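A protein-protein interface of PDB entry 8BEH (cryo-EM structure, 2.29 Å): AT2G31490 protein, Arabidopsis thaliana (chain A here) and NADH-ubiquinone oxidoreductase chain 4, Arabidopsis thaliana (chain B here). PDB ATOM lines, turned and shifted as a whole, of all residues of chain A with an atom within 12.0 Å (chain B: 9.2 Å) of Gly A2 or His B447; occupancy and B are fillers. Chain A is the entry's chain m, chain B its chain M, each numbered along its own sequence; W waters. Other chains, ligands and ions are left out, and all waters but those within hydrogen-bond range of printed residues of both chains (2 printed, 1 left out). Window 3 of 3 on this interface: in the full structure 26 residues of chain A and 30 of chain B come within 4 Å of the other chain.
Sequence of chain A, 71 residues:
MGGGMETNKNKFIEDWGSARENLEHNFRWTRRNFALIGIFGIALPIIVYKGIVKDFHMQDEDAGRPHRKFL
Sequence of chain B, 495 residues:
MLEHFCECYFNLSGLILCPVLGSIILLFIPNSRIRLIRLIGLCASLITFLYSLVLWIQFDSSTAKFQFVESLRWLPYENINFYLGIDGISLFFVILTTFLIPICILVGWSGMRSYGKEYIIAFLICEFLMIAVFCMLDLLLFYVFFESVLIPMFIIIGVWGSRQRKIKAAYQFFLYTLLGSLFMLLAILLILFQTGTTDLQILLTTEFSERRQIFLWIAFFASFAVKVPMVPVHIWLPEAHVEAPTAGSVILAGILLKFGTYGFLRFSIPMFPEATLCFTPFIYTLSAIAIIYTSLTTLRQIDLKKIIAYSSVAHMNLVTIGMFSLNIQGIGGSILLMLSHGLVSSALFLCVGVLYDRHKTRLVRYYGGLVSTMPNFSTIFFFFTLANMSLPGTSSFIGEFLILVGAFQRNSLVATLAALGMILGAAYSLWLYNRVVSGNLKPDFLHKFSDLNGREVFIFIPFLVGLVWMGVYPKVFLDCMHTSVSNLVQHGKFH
The backbone NH of Gly A2 is in hydrogen-bond range of a ring nitrogen (NE2) of His B447 (3.1 Å).
The backbone NH (N) of Thr A7 is in hydrogen-bond range of the backbone carbonyl oxygen (O) of His B359 (3.2 Å).
A ring nitrogen (ND1) of His B359 is in hydrogen-bond range of the backbone carbonyl oxygen (O) of Met A5 (2.9 Å).
The backbone NH (N) of Asn A8 sits at hydrogen-bond distance from the backbone carbonyl oxygen (O) of Phe B445 (3.0 Å).
Among the printed residues, pairs that only touch across the chains: Gly A4 with His B447, Gly A4 with Lys B448, Met A5 with Leu B446, Met A5 with Lys B448, Met A5 with Phe B449, Met A5 with Ser B450, Glu A6 with His B359, Thr A7 with Tyr B366, Thr A7 with Phe B445, Thr A7 with Leu B446, Asn A8 with Asp B444 and Lys A9 with Tyr B366.
His B447 touches two residues of chain A.
Pro B443 touches none of the printed residues of chain A.
Lys B448 touches just these residues of chain A: Gly A4 (3.97 Å) and Met A5 (3.6 Å).
Of chain A, only Met A5 comes within 4 Å of Phe B449.
Of the printed residues of chain B, Met A5 touches His B359 (2.9 Å), Leu B446 (3.5 Å), Lys B448 (3.6 Å), Phe B449 (3.6 Å) and Ser B450 (3.4 Å).
Of the printed residues of chain A, Phe B445 touches Thr A7 and Asn A8.
Of the printed residues of chain B, Thr A7 touches His B359, Tyr B366, Phe B445 and Leu B446.
Of the printed residues of chain B, Glu A6 touches His B359.
Of the printed residues of chain A, His B359 touches Met A5, Glu A6 and Thr A7.
The nearest printed residue of chain B that does not touch Gly A4 is Leu B446 (6.6 Å).
Printed residues of chain A that touch a printed residue of chain B: Gly A2, Gly A4, Met A5, Glu A6, Thr A7, Asn A8 and Lys A9.
Of the 15 printed residues of chain B, 9 touch a printed residue of chain A.
Along chain B the printed residues that touch a printed residue of chain A span positions 359 to 450.
Among the printed residues, 16 pairs touch across the chains.
Among the printed residues, no Asp or Glu carboxylate lies within 4 Å of a Lys or Arg side-chain nitrogen of the other chain.
Water W1 bridges NE2 of His B447 (2.5 Å) and O of Gly A2 (2.6 Å).
Water W2 lies within hydrogen-bond range of N of His B447 (3.0 Å), N of Lys B448 (3.0 Å) and O of Met A5 (3.1 Å).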
ATOM      1  N   GLY A   2      -0.117 -22.362 -12.661  1.00  0.00           N
ATOM      2  CA  GLY A   2       0.145 -22.524 -14.079  1.00  0.00           C
ATOM      3  C   GLY A   2       0.999 -23.739 -14.386  1.00  0.00           C
ATOM      4  O   GLY A   2       0.641 -24.573 -15.213  1.00  0.00           O
ATOM      5  N   GLY A   3       2.135 -23.835 -13.705  1.00  0.00           N
ATOM      6  CA  GLY A   3       3.038 -24.948 -13.899  1.00  0.00           C
ATOM      7  C   GLY A   3       3.385 -25.655 -12.609  1.00  0.00           C
ATOM      8  O   GLY A   3       3.868 -25.031 -11.661  1.00  0.00           O
ATOM      9  N   GLY A   4       3.071 -26.912 -12.540  1.00  0.00           N
ATOM     10  CA  GLY A   4       3.494 -27.683 -11.359  1.00  0.00           C
ATOM     11  C   GLY A   4       2.413 -28.017 -10.350  1.00  0.00           C
ATOM     12  O   GLY A   4       1.501 -27.233 -10.186  1.00  0.00           O
ATOM     13  N   MET A   5       2.571 -29.153  -9.686  1.00  0.00           N
ATOM     14  CA  MET A   5       1.685 -29.547  -8.569  1.00  0.00           C
ATOM     15  C   MET A   5       2.191 -28.865  -7.291  1.00  0.00           C
ATOM     16  O   MET A   5       1.414 -28.772  -6.370  1.00  0.00           O
ATOM     17  CB  MET A   5       1.660 -31.067  -8.405  1.00  0.00           C
ATOM     18  CG  MET A   5       0.963 -31.830  -9.484  1.00  0.00           C
ATOM     19  SD  MET A   5       0.990 -33.605  -9.119  1.00  0.00           S
ATOM     20  CE  MET A   5      -0.596 -33.774  -8.305  1.00  0.00           C
ATOM     21  N   GLU A   6       3.445 -28.381  -7.247  1.00  0.00           N
ATOM     22  CA  GLU A   6       3.907 -27.793  -5.998  1.00  0.00           C
ATOM     23  C   GLU A   6       3.049 -26.595  -5.615  1.00  0.00           C
ATOM     24  O   GLU A   6       2.554 -25.863  -6.475  1.00  0.00           O
ATOM     25  CB  GLU A   6       5.374 -27.374  -6.119  1.00  0.00           C
ATOM     26  CG  GLU A   6       6.345 -28.520  -5.965  1.00  0.00           C
ATOM     27  CD  GLU A   6       7.778 -28.061  -5.760  1.00  0.00           C
ATOM     28  OE1 GLU A   6       8.645 -28.435  -6.579  1.00  0.00           O
ATOM     29  OE2 GLU A   6       8.038 -27.329  -4.782  1.00  0.00           O
ATOM     30  N   THR A   7       2.854 -26.414  -4.313  1.00  0.00           N
ATOM     31  CA  THR A   7       2.083 -25.281  -3.833  1.00  0.00           C
ATOM     32  C   THR A   7       2.795 -23.975  -4.149  1.00  0.00           C
ATOM     33  O   THR A   7       4.025 -23.885  -4.128  1.00  0.00           O
ATOM     34  CB  THR A   7       1.836 -25.381  -2.324  1.00  0.00           C
ATOM     35  OG1 THR A   7       1.329 -24.133  -1.833  1.00  0.00           O
ATOM     36  CG2 THR A   7       3.101 -25.696  -1.606  1.00  0.00           C
ATOM     37  N   ASN A   8       2.001 -22.960  -4.461  1.00  0.00           N
ATOM     38  CA  ASN A   8       2.523 -21.612  -4.622  1.00  0.00           C
ATOM     39  C   ASN A   8       2.632 -20.990  -3.239  1.00  0.00           C
ATOM     40  O   ASN A   8       1.618 -20.668  -2.611  1.00  0.00           O
ATOM     41  CB  ASN A   8       1.625 -20.801  -5.546  1.00  0.00           C
ATOM     42  CG  ASN A   8       1.851 -21.137  -6.996  1.00  0.00           C
ATOM     43  OD1 ASN A   8       0.991 -21.716  -7.652  1.00  0.00           O
ATOM     44  ND2 ASN A   8       3.024 -20.791  -7.503  1.00  0.00           N
ATOM     45  N   LYS A   9       3.863 -20.847  -2.759  1.00  0.00           N
ATOM     46  CA  LYS A   9       4.100 -20.376  -1.403  1.00  0.00           C
ATOM     47  C   LYS A   9       3.574 -18.958  -1.219  1.00  0.00           C
ATOM     48  O   LYS A   9       3.640 -18.129  -2.129  1.00  0.00           O
ATOM     49  CB  LYS A   9       5.595 -20.409  -1.093  1.00  0.00           C
ATOM     50  CG  LYS A   9       6.052 -21.494  -0.149  1.00  0.00           C
ATOM     51  CD  LYS A   9       5.404 -22.834  -0.410  1.00  0.00           C
ATOM     52  CE  LYS A   9       6.267 -23.933   0.195  1.00  0.00           C
ATOM     53  NZ  LYS A   9       5.886 -25.307  -0.203  1.00  0.00           N
ATOM     54  N   HIS B 359       2.692 -32.020  -3.421  1.00  0.00           N
ATOM     55  CA  HIS B 359       2.558 -30.576  -3.144  1.00  0.00           C
ATOM     56  C   HIS B 359       3.706 -29.937  -2.371  1.00  0.00           C
ATOM     57  O   HIS B 359       3.705 -28.752  -2.351  1.00  0.00           O
ATOM     58  CB  HIS B 359       1.135 -30.348  -2.545  1.00  0.00           C
ATOM     59  CG  HIS B 359       0.087 -30.976  -3.390  1.00  0.00           C
ATOM     60  ND1 HIS B 359      -0.046 -30.678  -4.718  1.00  0.00           N
ATOM     61  CD2 HIS B 359      -0.844 -31.909  -3.116  1.00  0.00           C
ATOM     62  CE1 HIS B 359      -1.029 -31.370  -5.227  1.00  0.00           C
ATOM     63  NE2 HIS B 359      -1.536 -32.124  -4.270  1.00  0.00           N
ATOM     64  N   TYR B 366      -2.554 -24.473   3.525  1.00  0.00           N
ATOM     65  CA  TYR B 366      -2.524 -24.537   2.066  1.00  0.00           C
ATOM     66  C   TYR B 366      -3.545 -25.523   1.517  1.00  0.00           C
ATOM     67  O   TYR B 366      -4.040 -25.338   0.402  1.00  0.00           O
ATOM     68  CB  TYR B 366      -1.129 -24.917   1.575  1.00  0.00           C
ATOM     69  CG  TYR B 366      -0.103 -23.821   1.678  1.00  0.00           C
ATOM     70  CD1 TYR B 366      -0.328 -22.569   1.118  1.00  0.00           C
ATOM     71  CD2 TYR B 366       1.102 -24.044   2.324  1.00  0.00           C
ATOM     72  CE1 TYR B 366       0.619 -21.571   1.210  1.00  0.00           C
ATOM     73  CE2 TYR B 366       2.053 -23.058   2.422  1.00  0.00           C
ATOM     74  CZ  TYR B 366       1.813 -21.824   1.863  1.00  0.00           C
ATOM     75  OH  TYR B 366       2.771 -20.848   1.967  1.00  0.00           O
ATOM     76  N   GLY B 368      -7.124 -28.117   1.694  1.00  0.00           N
ATOM     77  CA  GLY B 368      -8.541 -27.864   1.847  1.00  0.00           C
ATOM     78  C   GLY B 368      -9.330 -28.221   0.606  1.00  0.00           C
ATOM     79  O   GLY B 368      -8.878 -27.979  -0.515  1.00  0.00           O
ATOM     80  N   LEU B 370      -9.913 -31.122  -0.606  1.00  0.00           N
ATOM     81  CA  LEU B 370      -9.329 -32.239  -1.339  1.00  0.00           C
ATOM     82  C   LEU B 370     -10.318 -33.371  -1.606  1.00  0.00           C
ATOM     83  O   LEU B 370     -10.018 -34.242  -2.427  1.00  0.00           O
ATOM     84  CB  LEU B 370      -8.117 -32.783  -0.579  1.00  0.00           C
ATOM     85  CG  LEU B 370      -6.814 -31.977  -0.654  1.00  0.00           C
ATOM     86  CD1 LEU B 370      -5.693 -32.688   0.094  1.00  0.00           C
ATOM     87  CD2 LEU B 370      -6.411 -31.689  -2.092  1.00  0.00           C
ATOM     88  N   THR B 373     -11.120 -33.450  -5.350  1.00  0.00           N
ATOM     89  CA  THR B 373     -10.110 -33.845  -6.321  1.00  0.00           C
ATOM     90  C   THR B 373      -9.450 -35.180  -6.010  1.00  0.00           C
ATOM     91  O   THR B 373      -8.950 -35.823  -6.934  1.00  0.00           O
ATOM     92  CB  THR B 373      -9.011 -32.775  -6.456  1.00  0.00           C
ATOM     93  OG1 THR B 373      -8.388 -32.528  -5.189  1.00  0.00           O
ATOM     94  CG2 THR B 373      -9.589 -31.475  -7.000  1.00  0.00           C
ATOM     95  N   LEU B 441     -11.673 -25.855  -2.394  1.00  0.00           N
ATOM     96  CA  LEU B 441     -10.313 -25.742  -2.882  1.00  0.00           C
ATOM     97  C   LEU B 441      -9.840 -24.295  -2.799  1.00  0.00           C
ATOM     98  O   LEU B 441     -10.631 -23.351  -2.756  1.00  0.00           O
ATOM     99  CB  LEU B 441     -10.209 -26.246  -4.318  1.00  0.00           C
ATOM    100  CG  LEU B 441     -10.590 -27.703  -4.572  1.00  0.00           C
ATOM    101  CD1 LEU B 441     -11.012 -27.886  -6.024  1.00  0.00           C
ATOM    102  CD2 LEU B 441      -9.452 -28.640  -4.200  1.00  0.00           C
ATOM    103  N   LYS B 442      -8.522 -24.130  -2.759  1.00  0.00           N
ATOM    104  CA  LYS B 442      -7.878 -22.821  -2.755  1.00  0.00           C
ATOM    105  C   LYS B 442      -6.930 -22.790  -3.947  1.00  0.00           C
ATOM    106  O   LYS B 442      -5.725 -23.049  -3.811  1.00  0.00           O
ATOM    107  CB  LYS B 442      -7.175 -22.547  -1.428  1.00  0.00           C
ATOM    108  CG  LYS B 442      -8.050 -22.833  -0.219  1.00  0.00           C
ATOM    109  CD  LYS B 442      -7.252 -23.248   0.992  1.00  0.00           C
ATOM    110  CE  LYS B 442      -8.154 -23.371   2.210  1.00  0.00           C
ATOM    111  NZ  LYS B 442      -7.403 -23.677   3.446  1.00  0.00           N
ATOM    112  N   PRO B 443      -7.449 -22.486  -5.139  1.00  0.00           N
ATOM    113  CA  PRO B 443      -6.637 -22.613  -6.359  1.00  0.00           C
ATOM    114  C   PRO B 443      -5.426 -21.693  -6.411  1.00  0.00           C
ATOM    115  O   PRO B 443      -4.493 -21.980  -7.169  1.00  0.00           O
ATOM    116  CB  PRO B 443      -7.638 -22.302  -7.478  1.00  0.00           C
ATOM    117  CG  PRO B 443      -8.737 -21.554  -6.818  1.00  0.00           C
ATOM    118  CD  PRO B 443      -8.832 -22.079  -5.431  1.00  0.00           C
ATOM    119  N   ASP B 444      -5.393 -20.613  -5.629  1.00  0.00           N
ATOM    120  CA  ASP B 444      -4.197 -19.778  -5.584  1.00  0.00           C
ATOM    121  C   ASP B 444      -3.014 -20.479  -4.927  1.00  0.00           C
ATOM    122  O   ASP B 444      -1.873 -20.073  -5.155  1.00  0.00           O
ATOM    123  CB  ASP B 444      -4.480 -18.466  -4.856  1.00  0.00           C
ATOM    124  CG  ASP B 444      -5.248 -17.485  -5.709  1.00  0.00           C
ATOM    125  OD1 ASP B 444      -6.491 -17.575  -5.744  1.00  0.00           O
ATOM    126  OD2 ASP B 444      -4.613 -16.619  -6.343  1.00  0.00           O
ATOM    127  N   PHE B 445      -3.253 -21.510  -4.117  1.00  0.00           N
ATOM    128  CA  PHE B 445      -2.170 -22.328  -3.584  1.00  0.00           C
ATOM    129  C   PHE B 445      -1.975 -23.617  -4.369  1.00  0.00           C
ATOM    130  O   PHE B 445      -0.859 -23.921  -4.792  1.00  0.00           O
ATOM    131  CB  PHE B 445      -2.406 -22.665  -2.106  1.00  0.00           C
ATOM    132  CG  PHE B 445      -2.725 -21.481  -1.252  1.00  0.00           C
ATOM    133  CD1 PHE B 445      -1.992 -20.310  -1.363  1.00  0.00           C
ATOM    134  CD2 PHE B 445      -3.724 -21.552  -0.298  1.00  0.00           C
ATOM    135  CE1 PHE B 445      -2.277 -19.226  -0.567  1.00  0.00           C
ATOM    136  CE2 PHE B 445      -4.008 -20.470   0.504  1.00  0.00           C
ATOM    137  CZ  PHE B 445      -3.285 -19.309   0.370  1.00  0.00           C
ATOM    138  N   LEU B 446      -3.026 -24.353  -4.637  1.00  0.00           N
ATOM    139  CA  LEU B 446      -2.960 -25.651  -5.298  1.00  0.00           C
ATOM    140  C   LEU B 446      -4.081 -25.706  -6.334  1.00  0.00           C
ATOM    141  O   LEU B 446      -5.201 -25.440  -5.980  1.00  0.00           O
ATOM    142  CB  LEU B 446      -3.067 -26.745  -4.219  1.00  0.00           C
ATOM    143  CG  LEU B 446      -1.896 -26.894  -3.254  1.00  0.00           C
ATOM    144  CD1 LEU B 446      -2.254 -27.811  -2.097  1.00  0.00           C
ATOM    145  CD2 LEU B 446      -0.664 -27.400  -3.974  1.00  0.00           C
ATOM    146  N   HIS B 447      -3.784 -26.134  -7.530  1.00  0.00           N
ATOM    147  CA  HIS B 447      -4.754 -26.136  -8.644  1.00  0.00           C
ATOM    148  C   HIS B 447      -4.579 -27.411  -9.463  1.00  0.00           C
ATOM    149  O   HIS B 447      -5.422 -27.696 -10.251  1.00  0.00           O
ATOM    150  CB  HIS B 447      -4.643 -24.819  -9.434  1.00  0.00           C
ATOM    151  CG  HIS B 447      -3.367 -24.764 -10.184  1.00  0.00           C
ATOM    152  ND1 HIS B 447      -2.159 -24.810  -9.554  1.00  0.00           N
ATOM    153  CD2 HIS B 447      -3.100 -24.772 -11.495  1.00  0.00           C
ATOM    154  CE1 HIS B 447      -1.192 -24.781 -10.431  1.00  0.00           C
ATOM    155  NE2 HIS B 447      -1.742 -24.740 -11.612  1.00  0.00           N
ATOM    156  N   LYS B 448      -3.506 -28.122  -9.252  1.00  0.00           N
ATOM    157  CA  LYS B 448      -3.233 -29.384  -9.965  1.00  0.00           C
ATOM    158  C   LYS B 448      -3.209 -30.561  -8.969  1.00  0.00           C
ATOM    159  O   LYS B 448      -2.532 -30.493  -8.013  1.00  0.00           O
ATOM    160  CB  LYS B 448      -2.032 -29.179 -10.888  1.00  0.00           C
ATOM    161  CG  LYS B 448      -1.491 -30.368 -11.638  1.00  0.00           C
ATOM    162  CD  LYS B 448      -0.302 -29.977 -12.488  1.00  0.00           C
ATOM    163  CE  LYS B 448      -0.662 -28.973 -13.557  1.00  0.00           C
ATOM    164  NZ  LYS B 448      -1.401 -29.626 -14.663  1.00  0.00           N
ATOM    165  N   PHE B 449      -3.928 -31.619  -9.287  1.00  0.00           N
ATOM    166  CA  PHE B 449      -4.137 -32.726  -8.323  1.00  0.00           C
ATOM    167  C   PHE B 449      -4.075 -34.090  -8.997  1.00  0.00           C
ATOM    168  O   PHE B 449      -4.317 -34.232 -10.144  1.00  0.00           O
ATOM    169  CB  PHE B 449      -5.417 -32.525  -7.463  1.00  0.00           C
ATOM    170  CG  PHE B 449      -5.594 -31.189  -6.806  1.00  0.00           C
ATOM    171  CD1 PHE B 449      -6.168 -30.136  -7.495  1.00  0.00           C
ATOM    172  CD2 PHE B 449      -5.213 -31.003  -5.490  1.00  0.00           C
ATOM    173  CE1 PHE B 449      -6.329 -28.909  -6.883  1.00  0.00           C
ATOM    174  CE2 PHE B 449      -5.382 -29.776  -4.883  1.00  0.00           C
ATOM    175  CZ  PHE B 449      -5.937 -28.734  -5.578  1.00  0.00           C
ATOM    176  N   SER B 450      -3.738 -35.080  -8.207  1.00  0.00           N
ATOM    177  CA  SER B 450      -3.756 -36.470  -8.635  1.00  0.00           C
ATOM    178  C   SER B 450      -4.138 -37.339  -7.449  1.00  0.00           C
ATOM    179  O   SER B 450      -3.519 -37.242  -6.387  1.00  0.00           O
ATOM    180  CB  SER B 450      -2.394 -36.904  -9.188  1.00  0.00           C
ATOM    181  OG  SER B 450      -2.512 -38.098  -9.929  1.00  0.00           O
HETATM  182  O   HOH W   1      -1.655 -25.148 -14.080  1.00  0.00           O
HETATM  183  O   HOH W   2      -1.028 -27.296  -7.692  1.00  0.00           O
